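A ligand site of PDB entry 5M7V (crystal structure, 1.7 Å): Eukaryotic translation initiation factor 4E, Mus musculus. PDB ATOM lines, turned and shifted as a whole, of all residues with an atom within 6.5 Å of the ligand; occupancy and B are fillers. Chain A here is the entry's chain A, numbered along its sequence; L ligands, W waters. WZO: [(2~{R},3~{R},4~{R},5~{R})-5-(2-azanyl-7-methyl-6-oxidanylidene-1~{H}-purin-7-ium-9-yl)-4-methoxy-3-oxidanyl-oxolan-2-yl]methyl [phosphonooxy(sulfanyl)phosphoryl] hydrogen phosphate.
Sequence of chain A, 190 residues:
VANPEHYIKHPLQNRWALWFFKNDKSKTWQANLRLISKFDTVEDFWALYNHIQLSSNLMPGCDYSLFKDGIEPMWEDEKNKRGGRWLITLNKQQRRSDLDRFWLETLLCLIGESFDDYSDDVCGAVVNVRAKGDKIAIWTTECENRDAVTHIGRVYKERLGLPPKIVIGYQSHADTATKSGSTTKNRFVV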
ATOM      1  N   PHE A  21       1.280  12.848   6.434  1.00  0.00           N
ATOM      2  CA  PHE A  21       0.121  12.782   7.318  1.00  0.00           C
ATOM      3  C   PHE A  21      -0.656  11.534   6.958  1.00  0.00           C
ATOM      4  O   PHE A  21      -0.953  11.303   5.790  1.00  0.00           O
ATOM      5  CB  PHE A  21      -0.767  14.033   7.163  1.00  0.00           C
ATOM      6  CG  PHE A  21      -2.003  14.012   8.037  1.00  0.00           C
ATOM      7  CD1 PHE A  21      -1.994  14.638   9.263  1.00  0.00           C
ATOM      8  CD2 PHE A  21      -3.163  13.399   7.610  1.00  0.00           C
ATOM      9  CE1 PHE A  21      -3.109  14.640  10.063  1.00  0.00           C
ATOM     10  CE2 PHE A  21      -4.294  13.390   8.422  1.00  0.00           C
ATOM     11  CZ  PHE A  21      -4.262  14.008   9.645  1.00  0.00           C
ATOM     12  N   TRP A  29      -5.054  15.325  15.164  1.00  0.00           N
ATOM     13  CA  TRP A  29      -4.505  15.702  13.873  1.00  0.00           C
ATOM     14  C   TRP A  29      -2.994  15.957  13.960  1.00  0.00           C
ATOM     15  O   TRP A  29      -2.229  15.468  13.122  1.00  0.00           O
ATOM     16  CB  TRP A  29      -5.235  16.937  13.335  1.00  0.00           C
ATOM     17  CG  TRP A  29      -4.755  17.378  11.986  1.00  0.00           C
ATOM     18  CD1 TRP A  29      -5.247  16.968  10.788  1.00  0.00           C
ATOM     19  CD2 TRP A  29      -3.691  18.293  11.704  1.00  0.00           C
ATOM     20  NE1 TRP A  29      -4.557  17.567   9.760  1.00  0.00           N
ATOM     21  CE2 TRP A  29      -3.584  18.388  10.297  1.00  0.00           C
ATOM     22  CE3 TRP A  29      -2.813  19.043  12.497  1.00  0.00           C
ATOM     23  CZ2 TRP A  29      -2.651  19.199   9.670  1.00  0.00           C
ATOM     24  CZ3 TRP A  29      -1.875  19.846  11.869  1.00  0.00           C
ATOM     25  CH2 TRP A  29      -1.790  19.915  10.478  1.00  0.00           C
ATOM     26  N   GLN A  30      -2.547  16.664  15.007  1.00  0.00           N
ATOM     27  CA  GLN A  30      -1.131  16.987  15.107  1.00  0.00           C
ATOM     28  C   GLN A  30      -0.276  15.736  15.327  1.00  0.00           C
ATOM     29  O   GLN A  30       0.841  15.644  14.822  1.00  0.00           O
ATOM     30  CB  GLN A  30      -0.890  18.000  16.219  1.00  0.00           C
ATOM     31  CG  GLN A  30       0.505  18.627  16.148  1.00  0.00           C
ATOM     32  CD  GLN A  30       0.755  19.635  17.252  1.00  0.00           C
ATOM     33  OE1 GLN A  30      -0.167  20.305  17.716  1.00  0.00           O
ATOM     34  NE2 GLN A  30       2.015  19.736  17.676  1.00  0.00           N
ATOM     35  N   GLY A  61      -7.002  10.086   2.783  1.00  0.00           N
ATOM     36  CA  GLY A  61      -6.763  10.599   4.104  1.00  0.00           C
ATOM     37  C   GLY A  61      -5.327  10.978   4.396  1.00  0.00           C
ATOM     38  O   GLY A  61      -5.036  11.483   5.495  1.00  0.00           O
ATOM     39  N   ASP A  63      -1.654  13.058   3.526  1.00  0.00           N
ATOM     40  CA  ASP A  63      -1.084  14.265   2.908  1.00  0.00           C
ATOM     41  C   ASP A  63       0.419  14.134   2.775  1.00  0.00           C
ATOM     42  O   ASP A  63       1.075  13.481   3.586  1.00  0.00           O
ATOM     43  CB  ASP A  63      -1.356  15.543   3.737  1.00  0.00           C
ATOM     44  CG  ASP A  63      -2.770  15.653   4.233  1.00  0.00           C
ATOM     45  OD1 ASP A  63      -3.668  15.151   3.552  1.00  0.00           O
ATOM     46  OD2 ASP A  63      -2.981  16.268   5.290  1.00  0.00           O
ATOM     47  N   PRO A  73       3.908  22.494   8.887  1.00  0.00           N
ATOM     48  CA  PRO A  73       2.777  22.554   7.941  1.00  0.00           C
ATOM     49  C   PRO A  73       1.413  22.645   8.617  1.00  0.00           C
ATOM     50  O   PRO A  73       0.504  21.848   8.340  1.00  0.00           O
ATOM     51  CB  PRO A  73       2.941  21.237   7.163  1.00  0.00           C
ATOM     52  CG  PRO A  73       3.594  20.327   8.115  1.00  0.00           C
ATOM     53  CD  PRO A  73       4.573  21.182   8.866  1.00  0.00           C
ATOM     54  N   MET A  74       1.256  23.613   9.510  1.00  0.00           N
ATOM     55  CA  MET A  74       0.025  23.779  10.265  1.00  0.00           C
ATOM     56  C   MET A  74      -0.282  25.256  10.413  1.00  0.00           C
ATOM     57  O   MET A  74       0.615  26.100  10.410  1.00  0.00           O
ATOM     58  CB  MET A  74       0.127  23.102  11.639  1.00  0.00           C
ATOM     59  CG  MET A  74       1.115  23.766  12.571  1.00  0.00           C
ATOM     60  SD  MET A  74       1.088  22.901  14.143  1.00  0.00           S
ATOM     61  CE  MET A  74       1.281  21.250  13.552  1.00  0.00           C
ATOM     62  N   TRP A  75      -1.583  25.559  10.554  1.00  0.00           N
ATOM     63  CA  TRP A  75      -1.992  26.955  10.705  1.00  0.00           C
ATOM     64  C   TRP A  75      -1.291  27.638  11.867  1.00  0.00           C
ATOM     65  O   TRP A  75      -1.092  28.846  11.827  1.00  0.00           O
ATOM     66  CB  TRP A  75      -3.507  27.077  10.923  1.00  0.00           C
ATOM     67  CG  TRP A  75      -4.370  26.279  10.016  1.00  0.00           C
ATOM     68  CD1 TRP A  75      -4.202  26.064   8.670  1.00  0.00           C
ATOM     69  CD2 TRP A  75      -5.550  25.573  10.385  1.00  0.00           C
ATOM     70  NE1 TRP A  75      -5.221  25.283   8.182  1.00  0.00           N
ATOM     71  CE2 TRP A  75      -6.059  24.958   9.224  1.00  0.00           C
ATOM     72  CE3 TRP A  75      -6.228  25.400  11.592  1.00  0.00           C
ATOM     73  CZ2 TRP A  75      -7.199  24.192   9.242  1.00  0.00           C
ATOM     74  CZ3 TRP A  75      -7.345  24.649  11.603  1.00  0.00           C
ATOM     75  CH2 TRP A  75      -7.832  24.050  10.435  1.00  0.00           C
ATOM     76  N   GLU A  76      -0.949  26.890  12.912  1.00  0.00           N
ATOM     77  CA  GLU A  76      -0.546  27.539  14.151  1.00  0.00           C
ATOM     78  C   GLU A  76       0.866  28.092  14.084  1.00  0.00           C
ATOM     79  O   GLU A  76       1.221  28.949  14.907  1.00  0.00           O
ATOM     80  CB  GLU A  76      -0.722  26.572  15.322  1.00  0.00           C
ATOM     81  CG  GLU A  76      -2.181  26.307  15.641  1.00  0.00           C
ATOM     82  CD  GLU A  76      -2.721  25.106  14.924  1.00  0.00           C
ATOM     83  OE1 GLU A  76      -3.506  24.358  15.539  1.00  0.00           O
ATOM     84  OE2 GLU A  76      -2.344  24.895  13.750  1.00  0.00           O
ATOM     85  N   ARG A  85      -3.790  30.161   1.510  1.00  0.00           N
ATOM     86  CA  ARG A  85      -3.382  29.207   0.487  1.00  0.00           C
ATOM     87  C   ARG A  85      -4.024  29.509  -0.860  1.00  0.00           C
ATOM     88  O   ARG A  85      -5.200  29.853  -0.912  1.00  0.00           O
ATOM     89  CB  ARG A  85      -3.733  27.756   0.904  1.00  0.00           C
ATOM     90  CG  ARG A  85      -5.239  27.452   1.012  1.00  0.00           C
ATOM     91  CD  ARG A  85      -5.465  25.988   1.402  1.00  0.00           C
ATOM     92  NE  ARG A  85      -6.879  25.694   1.663  1.00  0.00           N
ATOM     93  CZ  ARG A  85      -7.346  24.503   2.045  1.00  0.00           C
ATOM     94  NH1 ARG A  85      -6.512  23.481   2.183  1.00  0.00           N
ATOM     95  NH2 ARG A  85      -8.639  24.340   2.270  1.00  0.00           N
ATOM     96  N   ASN A 128      -3.477  16.983  -0.443  1.00  0.00           N
ATOM     97  CA  ASN A 128      -4.387  16.123   0.294  1.00  0.00           C
ATOM     98  C   ASN A 128      -4.988  15.093  -0.649  1.00  0.00           C
ATOM     99  O   ASN A 128      -5.616  15.455  -1.642  1.00  0.00           O
ATOM    100  CB  ASN A 128      -5.502  16.924   0.967  1.00  0.00           C
ATOM    101  CG  ASN A 128      -5.005  18.105   1.762  1.00  0.00           C
ATOM    102  OD1 ASN A 128      -5.229  19.254   1.392  1.00  0.00           O
ATOM    103  ND2 ASN A 128      -4.344  17.823   2.869  1.00  0.00           N
ATOM    104  N   ARG A 130      -7.829  12.603  -1.057  1.00  0.00           N
ATOM    105  CA  ARG A 130      -9.133  12.434  -0.420  1.00  0.00           C
ATOM    106  C   ARG A 130     -10.091  11.753  -1.379  1.00  0.00           C
ATOM    107  O   ARG A 130     -10.127  12.073  -2.577  1.00  0.00           O
ATOM    108  CB  ARG A 130      -9.707  13.784   0.044  1.00  0.00           C
ATOM    109  CG  ARG A 130      -8.836  14.500   1.054  1.00  0.00           C
ATOM    110  CD  ARG A 130      -8.835  13.768   2.406  1.00  0.00           C
ATOM    111  NE  ARG A 130      -8.191  14.572   3.419  1.00  0.00           N
ATOM    112  CZ  ARG A 130      -6.863  14.653   3.590  1.00  0.00           C
ATOM    113  NH1 ARG A 130      -6.035  13.964   2.828  1.00  0.00           N
ATOM    114  NH2 ARG A 130      -6.381  15.424   4.548  1.00  0.00           N
ATOM    115  N   GLY A 133     -12.261  14.117  -3.372  1.00  0.00           N
ATOM    116  CA  GLY A 133     -11.619  15.065  -4.243  1.00  0.00           C
ATOM    117  C   GLY A 133     -10.297  15.492  -3.640  1.00  0.00           C
ATOM    118  O   GLY A 133     -10.231  15.905  -2.473  1.00  0.00           O
ATOM    119  N   ASP A 134      -9.227  15.375  -4.409  1.00  0.00           N
ATOM    120  CA  ASP A 134      -7.907  15.769  -3.946  1.00  0.00           C
ATOM    121  C   ASP A 134      -7.737  17.281  -3.951  1.00  0.00           C
ATOM    122  O   ASP A 134      -8.440  18.007  -4.666  1.00  0.00           O
ATOM    123  CB  ASP A 134      -6.851  15.151  -4.840  1.00  0.00           C
ATOM    124  CG  ASP A 134      -6.951  13.664  -4.897  1.00  0.00           C
ATOM    125  OD1 ASP A 134      -7.228  13.041  -3.840  1.00  0.00           O
ATOM    126  OD2 ASP A 134      -6.739  13.098  -5.983  1.00  0.00           O
ATOM    127  N   LYS A 135      -6.763  17.759  -3.161  1.00  0.00           N
ATOM    128  CA  LYS A 135      -6.445  19.176  -3.092  1.00  0.00           C
ATOM    129  C   LYS A 135      -4.946  19.342  -3.159  1.00  0.00           C
ATOM    130  O   LYS A 135      -4.206  18.559  -2.562  1.00  0.00           O
ATOM    131  CB  LYS A 135      -6.973  19.837  -1.788  1.00  0.00           C
ATOM    132  CG  LYS A 135      -8.477  19.761  -1.599  1.00  0.00           C
ATOM    133  CD  LYS A 135      -8.967  20.816  -0.593  1.00  0.00           C
ATOM    134  CE  LYS A 135     -10.364  20.504  -0.085  1.00  0.00           C
ATOM    135  NZ  LYS A 135     -10.903  21.652   0.709  1.00  0.00           N
ATOM    136  N   TRP A 139       0.991  27.438   0.330  1.00  0.00           N
ATOM    137  CA  TRP A 139       0.753  28.273   1.498  1.00  0.00           C
ATOM    138  C   TRP A 139       1.680  29.488   1.464  1.00  0.00           C
ATOM    139  O   TRP A 139       2.891  29.355   1.235  1.00  0.00           O
ATOM    140  CB  TRP A 139       0.972  27.496   2.800  1.00  0.00           C
ATOM    141  CG  TRP A 139      -0.070  26.475   3.090  1.00  0.00           C
ATOM    142  CD1 TRP A 139      -0.879  25.821   2.190  1.00  0.00           C
ATOM    143  CD2 TRP A 139      -0.419  25.967   4.375  1.00  0.00           C
ATOM    144  NE1 TRP A 139      -1.707  24.947   2.845  1.00  0.00           N
ATOM    145  CE2 TRP A 139      -1.454  25.023   4.195  1.00  0.00           C
ATOM    146  CE3 TRP A 139       0.037  26.216   5.673  1.00  0.00           C
ATOM    147  CZ2 TRP A 139      -2.029  24.320   5.254  1.00  0.00           C
ATOM    148  CZ3 TRP A 139      -0.540  25.525   6.724  1.00  0.00           C
ATOM    149  CH2 TRP A 139      -1.564  24.601   6.510  1.00  0.00           C
ATOM    150  N   THR A 176     -10.444  29.311   6.972  1.00  0.00           N
ATOM    151  CA  THR A 176     -10.522  27.864   6.847  1.00  0.00           C
ATOM    152  C   THR A 176     -10.640  27.196   8.210  1.00  0.00           C
ATOM    153  O   THR A 176     -11.266  26.133   8.326  1.00  0.00           O
ATOM    154  CB  THR A 176      -9.288  27.314   6.110  1.00  0.00           C
ATOM    155  OG1 THR A 176      -8.938  28.179   5.021  1.00  0.00           O
ATOM    156  CG2 THR A 176      -9.574  25.906   5.559  1.00  0.00           C
ATOM    157  N   ALA A 177     -10.046  27.798   9.244  1.00  0.00           N
ATOM    158  CA  ALA A 177      -9.990  27.175  10.556  1.00  0.00           C
ATOM    159  C   ALA A 177     -11.330  27.209  11.271  1.00  0.00           C
ATOM    160  O   ALA A 177     -11.629  26.301  12.054  1.00  0.00           O
ATOM    161  CB  ALA A 177      -8.919  27.862  11.409  1.00  0.00           C
HETATM  162  C2  WZO L   1      -4.889  21.921  13.177  1.00  0.00           C
HETATM  163  C8  WZO L   1      -6.291  20.489   9.199  1.00  0.00           C
HETATM  164  C4  WZO L   1      -5.872  20.983  11.299  1.00  0.00           C
HETATM  165  C5  WZO L   1      -4.980  21.639  10.482  1.00  0.00           C
HETATM  166  C6  WZO L   1      -4.024  22.472  11.050  1.00  0.00           C
HETATM  167  OC2 WZO L   1      -7.616  17.375   6.090  1.00  0.00           O
HETATM  168  PC  WZO L   1      -8.206  18.763   6.035  1.00  0.00           P
HETATM  169  OC1 WZO L   1      -7.412  19.891   5.429  1.00  0.00           O
HETATM  170  OBC WZO L   1      -9.644  18.791   5.313  1.00  0.00           O
HETATM  171  PB  WZO L   1     -10.097  17.867   4.083  1.00  0.00           P
HETATM  172  OB  WZO L   1     -10.007  16.447   4.479  1.00  0.00           O
HETATM  173  SB  WZO L   1      -9.041  18.090   2.342  1.00  0.00           S
HETATM  174  OAB WZO L   1     -11.628  18.349   3.895  1.00  0.00           O
HETATM  175  PA  WZO L   1     -12.108  19.876   4.105  1.00  0.00           P
HETATM  176  OA2 WZO L   1     -10.877  20.745   3.922  1.00  0.00           O
HETATM  177  OA1 WZO L   1     -12.671  19.897   5.517  1.00  0.00           O
HETATM  178  OA3 WZO L   1     -13.224  20.059   2.964  1.00  0.00           O
HETATM  179  O5' WZO L   1      -8.667  19.211   7.518  1.00  0.00           O
HETATM  180  C5' WZO L   1      -9.640  18.385   8.156  1.00  0.00           C
HETATM  181  C4' WZO L   1      -9.494  18.638   9.632  1.00  0.00           C
HETATM  182  C3' WZO L   1      -9.802  20.086   9.944  1.00  0.00           C
HETATM  183  O3' WZO L   1     -11.199  20.287  10.177  1.00  0.00           O
HETATM  184  C2' WZO L   1      -8.991  20.311  11.196  1.00  0.00           C
HETATM  185  O2' WZO L   1      -9.773  19.818  12.276  1.00  0.00           O
HETATM  186  CM2 WZO L   1      -9.253  20.208  13.550  1.00  0.00           C
HETATM  187  C1' WZO L   1      -7.777  19.420  10.994  1.00  0.00           C
HETATM  188  O4' WZO L   1      -8.133  18.446  10.026  1.00  0.00           O
HETATM  189  N9  WZO L   1      -6.667  20.263  10.499  1.00  0.00           N
HETATM  190  N3  WZO L   1      -5.819  21.117  12.642  1.00  0.00           N
HETATM  191  N2  WZO L   1      -4.820  22.091  14.504  1.00  0.00           N
HETATM  192  N1  WZO L   1      -4.000  22.586  12.395  1.00  0.00           N
HETATM  193  O6  WZO L   1      -3.089  23.154  10.344  1.00  0.00           O
HETATM  194  N7  WZO L   1      -5.237  21.341   9.204  1.00  0.00           N
HETATM  195  CM7 WZO L   1      -4.518  21.831   8.000  1.00  0.00           C
HETATM  196  O   HOH W   1     -12.329  14.399   4.675  1.00  0.00           O
HETATM  197  O   HOH W   2      -4.773  17.056   7.041  1.00  0.00           O
HETATM  198  O   HOH W   3      -8.243  22.214   5.829  1.00  0.00           O
HETATM  199  O   HOH W   4     -10.639  14.874   6.534  1.00  0.00           O
HETATM  200  O   HOH W   5      -6.713  20.782   3.027  1.00  0.00           O
HETATM  201  O   HOH W   6      -7.207  15.198   7.727  1.00  0.00           O
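The guanidinium group (NH2) of Arg 130 lies within salt-bridge range of an oxygen (OC2) of the ligand. N2 of the ligand sits at hydrogen-bond distance from OE1 of Glu 76, 2.8 Å away. The backbone NH of Trp 75 sits at hydrogen-bond distance from an oxygen (O6) of the ligand. An oxygen (OA2) of the ligand is in salt-bridge range of the side-chain amino group (NZ) of Lys 135 (3.3 Å).
NH1 of Arg 130 is in salt-bridge range of OD1 of Asp 63 (2.7 Å). N of Arg 130 lies within hydrogen-bond range of OD1 of Asp 134, at 2.9 Å. The backbone carbonyl oxygen (O) of Lys 135 sits at hydrogen-bond distance from the backbone NH (N) of Asn 128 (2.7 Å). The side-chain carboxylate (OD1) of Asp 63 lies within hydrogen-bond range of the side-chain amide nitrogen (ND2) of Asn 128 (2.8 Å).
Trp 29 touches the ligand (CD1 to O4', 3.3 Å). Met 74 touches the ligand (CA to O6, 3.2 Å). Asn 128 touches the ligand. Hydrophobic or aromatic side chains that line the ligand: Trp 29, Met 74 and Trp 75. The nearest printed residue that does not touch the ligand is Trp 139 (4.3 Å).
Water W5 lies within hydrogen-bond range of an oxygen (OC1) of the ligand (2.7 Å), the side-chain amide oxygen of Asn 128 (2.7 Å) and the guanidinium group of Arg 85 (2.8 Å). Water W6 lies within hydrogen-bond range of an oxygen (OC2) of the ligand and the guanidinium group of Arg 130. Water W2 lies within hydrogen-bond range of the side-chain carboxylate of Asp 63, the indole nitrogen of Trp 29, an oxygen (OC2) of the ligand and the guanidinium group of Arg 130.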
